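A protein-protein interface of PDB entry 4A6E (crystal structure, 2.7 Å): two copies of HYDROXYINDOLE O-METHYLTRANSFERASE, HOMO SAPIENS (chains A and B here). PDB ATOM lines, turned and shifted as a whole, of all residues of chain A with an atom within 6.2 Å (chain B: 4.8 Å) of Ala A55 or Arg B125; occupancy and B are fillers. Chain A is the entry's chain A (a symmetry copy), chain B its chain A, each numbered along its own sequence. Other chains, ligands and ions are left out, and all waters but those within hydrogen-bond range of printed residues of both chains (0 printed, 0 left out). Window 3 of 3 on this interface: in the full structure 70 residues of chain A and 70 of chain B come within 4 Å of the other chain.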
ATOM      1  N   GLU A  30      -4.334  17.303  25.816  1.00  0.00           N
ATOM      2  CA  GLU A  30      -4.144  17.551  24.387  1.00  0.00           C
ATOM      3  C   GLU A  30      -4.557  18.969  23.959  1.00  0.00           C
ATOM      4  O   GLU A  30      -3.983  19.494  23.011  1.00  0.00           O
ATOM      5  CB  GLU A  30      -4.915  16.502  23.558  1.00  0.00           C
ATOM      6  CG  GLU A  30      -4.332  15.088  23.583  1.00  0.00           C
ATOM      7  CD  GLU A  30      -5.310  13.928  23.426  1.00  0.00           C
ATOM      8  OE1 GLU A  30      -6.493  14.175  23.098  1.00  0.00           O
ATOM      9  OE2 GLU A  30      -4.894  12.764  23.635  1.00  0.00           O
ATOM     10  N   LEU A  31      -5.562  19.575  24.630  1.00  0.00           N
ATOM     11  CA  LEU A  31      -6.080  20.917  24.341  1.00  0.00           C
ATOM     12  C   LEU A  31      -5.404  21.990  25.204  1.00  0.00           C
ATOM     13  O   LEU A  31      -5.531  23.182  24.914  1.00  0.00           O
ATOM     14  CB  LEU A  31      -7.594  20.957  24.578  1.00  0.00           C
ATOM     15  CG  LEU A  31      -8.501  20.273  23.560  1.00  0.00           C
ATOM     16  CD1 LEU A  31      -9.858  20.014  24.165  1.00  0.00           C
ATOM     17  CD2 LEU A  31      -8.678  21.117  22.314  1.00  0.00           C
ATOM     18  N   VAL A  49     -12.146  29.697  28.113  1.00  0.00           N
ATOM     19  CA  VAL A  49     -11.423  28.433  27.939  1.00  0.00           C
ATOM     20  C   VAL A  49     -11.549  28.024  26.461  1.00  0.00           C
ATOM     21  O   VAL A  49     -10.529  27.821  25.797  1.00  0.00           O
ATOM     22  CB  VAL A  49     -11.927  27.337  28.934  1.00  0.00           C
ATOM     23  CG1 VAL A  49     -11.293  25.970  28.657  1.00  0.00           C
ATOM     24  CG2 VAL A  49     -11.689  27.755  30.386  1.00  0.00           C
ATOM     25  N   ALA A  50     -12.795  28.010  25.935  1.00  0.00           N
ATOM     26  CA  ALA A  50     -13.106  27.679  24.544  1.00  0.00           C
ATOM     27  C   ALA A  50     -12.271  28.509  23.599  1.00  0.00           C
ATOM     28  O   ALA A  50     -11.606  27.935  22.738  1.00  0.00           O
ATOM     29  CB  ALA A  50     -14.588  27.876  24.262  1.00  0.00           C
ATOM     30  N   ALA A  51     -12.216  29.838  23.822  1.00  0.00           N
ATOM     31  CA  ALA A  51     -11.424  30.748  22.997  1.00  0.00           C
ATOM     32  C   ALA A  51      -9.912  30.475  23.093  1.00  0.00           C
ATOM     33  O   ALA A  51      -9.254  30.362  22.059  1.00  0.00           O
ATOM     34  CB  ALA A  51     -11.736  32.192  23.346  1.00  0.00           C
ATOM     35  N   VAL A  53      -8.319  27.745  23.839  1.00  0.00           N
ATOM     36  CA  VAL A  53      -7.901  26.401  23.372  1.00  0.00           C
ATOM     37  C   VAL A  53      -8.369  26.099  21.924  1.00  0.00           C
ATOM     38  O   VAL A  53      -8.080  25.017  21.402  1.00  0.00           O
ATOM     39  CB  VAL A  53      -8.237  25.237  24.361  1.00  0.00           C
ATOM     40  CG1 VAL A  53      -7.733  25.524  25.768  1.00  0.00           C
ATOM     41  CG2 VAL A  53      -9.725  24.913  24.375  1.00  0.00           C
ATOM     42  N   ARG A  54      -9.075  27.067  21.283  1.00  0.00           N
ATOM     43  CA  ARG A  54      -9.644  26.960  19.933  1.00  0.00           C
ATOM     44  C   ARG A  54     -10.591  25.732  19.815  1.00  0.00           C
ATOM     45  O   ARG A  54     -10.349  24.819  19.018  1.00  0.00           O
ATOM     46  CB  ARG A  54      -8.555  26.996  18.828  1.00  0.00           C
ATOM     47  CG  ARG A  54      -7.993  28.378  18.504  1.00  0.00           C
ATOM     48  CD  ARG A  54      -6.664  28.680  19.191  1.00  0.00           C
ATOM     49  NE  ARG A  54      -6.175  30.022  18.845  1.00  0.00           N
ATOM     50  CZ  ARG A  54      -6.237  31.088  19.644  1.00  0.00           C
ATOM     51  NH1 ARG A  54      -6.735  30.981  20.871  1.00  0.00           N
ATOM     52  NH2 ARG A  54      -5.786  32.264  19.227  1.00  0.00           N
ATOM     53  N   ALA A  55     -11.648  25.708  20.655  1.00  0.00           N
ATOM     54  CA  ALA A  55     -12.656  24.643  20.684  1.00  0.00           C
ATOM     55  C   ALA A  55     -14.079  25.197  20.779  1.00  0.00           C
ATOM     56  O   ALA A  55     -14.276  26.415  20.891  1.00  0.00           O
ATOM     57  CB  ALA A  55     -12.385  23.688  21.831  1.00  0.00           C
ATOM     58  N   SER A  56     -15.069  24.290  20.713  1.00  0.00           N
ATOM     59  CA  SER A  56     -16.504  24.580  20.779  1.00  0.00           C
ATOM     60  C   SER A  56     -16.893  25.111  22.111  1.00  0.00           C
ATOM     61  O   SER A  56     -16.321  24.694  23.105  1.00  0.00           O
ATOM     62  CB  SER A  56     -17.292  23.294  20.594  1.00  0.00           C
ATOM     63  OG  SER A  56     -17.096  22.830  19.277  1.00  0.00           O
ATOM     64  N   ALA A  57     -17.932  25.936  22.154  1.00  0.00           N
ATOM     65  CA  ALA A  57     -18.512  26.404  23.396  1.00  0.00           C
ATOM     66  C   ALA A  57     -19.178  25.175  24.052  1.00  0.00           C
ATOM     67  O   ALA A  57     -18.908  24.899  25.227  1.00  0.00           O
ATOM     68  CB  ALA A  57     -19.547  27.480  23.107  1.00  0.00           C
ATOM     69  N   GLY A  59     -18.698  21.804  23.328  1.00  0.00           N
ATOM     70  CA  GLY A  59     -17.660  20.807  23.579  1.00  0.00           C
ATOM     71  C   GLY A  59     -16.868  21.136  24.827  1.00  0.00           C
ATOM     72  O   GLY A  59     -16.792  20.308  25.736  1.00  0.00           O
ATOM     73  N   THR A  60     -16.314  22.369  24.897  1.00  0.00           N
ATOM     74  CA  THR A  60     -15.540  22.881  26.044  1.00  0.00           C
ATOM     75  C   THR A  60     -16.340  22.726  27.348  1.00  0.00           C
ATOM     76  O   THR A  60     -15.838  22.104  28.284  1.00  0.00           O
ATOM     77  CB  THR A  60     -15.120  24.347  25.798  1.00  0.00           C
ATOM     78  OG1 THR A  60     -14.271  24.387  24.664  1.00  0.00           O
ATOM     79  CG2 THR A  60     -14.432  24.995  26.984  1.00  0.00           C
ATOM     80  N   ARG A 111      -2.981   8.835  22.485  1.00  0.00           N
ATOM     81  CA  ARG A 111      -2.701   8.855  21.054  1.00  0.00           C
ATOM     82  C   ARG A 111      -2.127   7.528  20.566  1.00  0.00           C
ATOM     83  O   ARG A 111      -2.381   7.139  19.411  1.00  0.00           O
ATOM     84  CB  ARG A 111      -1.771  10.019  20.682  1.00  0.00           C
ATOM     85  CG  ARG A 111      -2.322  11.400  21.027  1.00  0.00           C
ATOM     86  CD  ARG A 111      -1.239  12.451  20.893  1.00  0.00           C
ATOM     87  NE  ARG A 111      -1.743  13.801  21.146  1.00  0.00           N
ATOM     88  CZ  ARG A 111      -0.978  14.829  21.500  1.00  0.00           C
ATOM     89  NH1 ARG A 111       0.324  14.659  21.690  1.00  0.00           N
ATOM     90  NH2 ARG A 111      -1.514  16.026  21.700  1.00  0.00           N
ATOM     91  N   ALA B 121     -10.741  14.987  21.172  1.00  0.00           N
ATOM     92  CA  ALA B 121     -10.174  16.336  21.075  1.00  0.00           C
ATOM     93  C   ALA B 121     -10.756  17.043  19.847  1.00  0.00           C
ATOM     94  O   ALA B 121     -11.265  18.171  19.973  1.00  0.00           O
ATOM     95  CB  ALA B 121      -8.656  16.267  20.971  1.00  0.00           C
ATOM     96  N   ASP B 122     -10.762  16.338  18.687  1.00  0.00           N
ATOM     97  CA  ASP B 122     -11.292  16.867  17.435  1.00  0.00           C
ATOM     98  C   ASP B 122     -12.793  17.154  17.484  1.00  0.00           C
ATOM     99  O   ASP B 122     -13.198  18.223  17.042  1.00  0.00           O
ATOM    100  CB  ASP B 122     -10.898  15.988  16.242  1.00  0.00           C
ATOM    101  CG  ASP B 122      -9.413  16.061  15.900  1.00  0.00           C
ATOM    102  OD1 ASP B 122      -8.879  17.196  15.788  1.00  0.00           O
ATOM    103  OD2 ASP B 122      -8.787  14.988  15.732  1.00  0.00           O
ATOM    104  N   ALA B 123     -13.607  16.243  18.088  1.00  0.00           N
ATOM    105  CA  ALA B 123     -15.065  16.408  18.271  1.00  0.00           C
ATOM    106  C   ALA B 123     -15.329  17.623  19.154  1.00  0.00           C
ATOM    107  O   ALA B 123     -16.217  18.414  18.849  1.00  0.00           O
ATOM    108  CB  ALA B 123     -15.675  15.163  18.890  1.00  0.00           C
ATOM    109  N   VAL B 124     -14.500  17.804  20.202  1.00  0.00           N
ATOM    110  CA  VAL B 124     -14.562  18.954  21.100  1.00  0.00           C
ATOM    111  C   VAL B 124     -14.169  20.236  20.335  1.00  0.00           C
ATOM    112  O   VAL B 124     -14.911  21.212  20.393  1.00  0.00           O
ATOM    113  CB  VAL B 124     -13.772  18.712  22.421  1.00  0.00           C
ATOM    114  CG1 VAL B 124     -13.593  19.991  23.238  1.00  0.00           C
ATOM    115  CG2 VAL B 124     -14.445  17.621  23.254  1.00  0.00           C
ATOM    116  N   ARG B 125     -13.071  20.198  19.559  1.00  0.00           N
ATOM    117  CA  ARG B 125     -12.630  21.328  18.730  1.00  0.00           C
ATOM    118  C   ARG B 125     -13.686  21.790  17.701  1.00  0.00           C
ATOM    119  O   ARG B 125     -13.985  22.984  17.627  1.00  0.00           O
ATOM    120  CB  ARG B 125     -11.357  20.965  17.977  1.00  0.00           C
ATOM    121  CG  ARG B 125     -10.105  21.081  18.804  1.00  0.00           C
ATOM    122  CD  ARG B 125      -8.862  20.941  17.946  1.00  0.00           C
ATOM    123  NE  ARG B 125      -7.686  20.633  18.767  1.00  0.00           N
ATOM    124  CZ  ARG B 125      -7.184  19.412  18.928  1.00  0.00           C
ATOM    125  NH1 ARG B 125      -7.721  18.377  18.296  1.00  0.00           N
ATOM    126  NH2 ARG B 125      -6.119  19.224  19.693  1.00  0.00           N
ATOM    127  N   GLU B 126     -14.265  20.829  16.949  1.00  0.00           N
ATOM    128  CA  GLU B 126     -15.203  21.020  15.844  1.00  0.00           C
ATOM    129  C   GLU B 126     -16.671  21.115  16.217  1.00  0.00           C
ATOM    130  O   GLU B 126     -17.470  21.584  15.394  1.00  0.00           O
ATOM    131  CB  GLU B 126     -15.035  19.885  14.816  1.00  0.00           C
ATOM    132  CG  GLU B 126     -13.669  19.815  14.136  1.00  0.00           C
ATOM    133  CD  GLU B 126     -13.319  18.457  13.554  1.00  0.00           C
ATOM    134  OE1 GLU B 126     -14.185  17.849  12.882  1.00  0.00           O
ATOM    135  OE2 GLU B 126     -12.186  17.986  13.801  1.00  0.00           O
ATOM    136  N   GLY B 127     -17.038  20.585  17.387  1.00  0.00           N
ATOM    137  CA  GLY B 127     -18.423  20.544  17.851  1.00  0.00           C
ATOM    138  C   GLY B 127     -19.283  19.598  17.045  1.00  0.00           C
ATOM    139  O   GLY B 127     -20.504  19.755  16.982  1.00  0.00           O
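O of Val B124 is in hydrogen-bond range of OG of Ser A56 (2.9 Å).
The side-chain hydroxyl (OG) of Ser A56 sits at hydrogen-bond distance from the backbone NH (N) of Gly B127, at 2.9 Å.
The side-chain carboxylate (OD1) of Asp B122 lies within salt-bridge range of the guanidinium group (NH1) of Arg B125 (3.0 Å).
N of Ala A55 is in hydrogen-bond range of O of Ala A50 (3.0 Å).
O of Ala A51 is in hydrogen-bond range of NH1 of Arg A54.
O of Ser A56 is in hydrogen-bond range of OG1 of Thr A60 (2.6 Å).
Among the printed residues, pairs that only touch across the chains: Ser A56 with Arg B125, Ser A56 with Glu B126, Glu A30 with Ala B121, Leu A31 with Arg B125, Ala A55 with Arg B125, Arg A54 with Arg B125, Gly A59 with Val B124, Ala A55 with Val B124, Leu A31 with Val B124, Glu A30 with Arg B125 and Thr A60 with Val B124.
Ala A55 touches just these residues of chain B: Val B124 (3.8 Å) and Arg B125 (3.7 Å).
Arg B125 touches just these residues of chain A: Glu A30, Leu A31, Arg A54, Ala A55 and Ser A56.
Of the printed residues of chain A, Glu B126 touches Ser A56.
Of the printed residues of chain B, Thr A60 touches Val B124 (3.98 Å).
Ala A57 touches none of the printed residues of chain B.
The nearest printed residue of chain B that does not touch Ala A55 is Glu B126 (5.6 Å).
The nearest residue of chain A that does not touch Arg B125 is Val A53 (5.1 Å).
The nearest printed residue of chain A that does not touch Val B124 is Ala A57 (5.9 Å).
Of the 13 printed residues of chain A, 7 touch a printed residue of chain B.
Hydrophobic or aromatic side chains of chain B that line the printed part of chain A: Ala B121 and Val B124.
Along chain B the printed residues that touch a printed residue of chain A span positions 121 to 127.
Among the printed residues, 13 pairs touch across the chains.
No position is printed for both chains.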
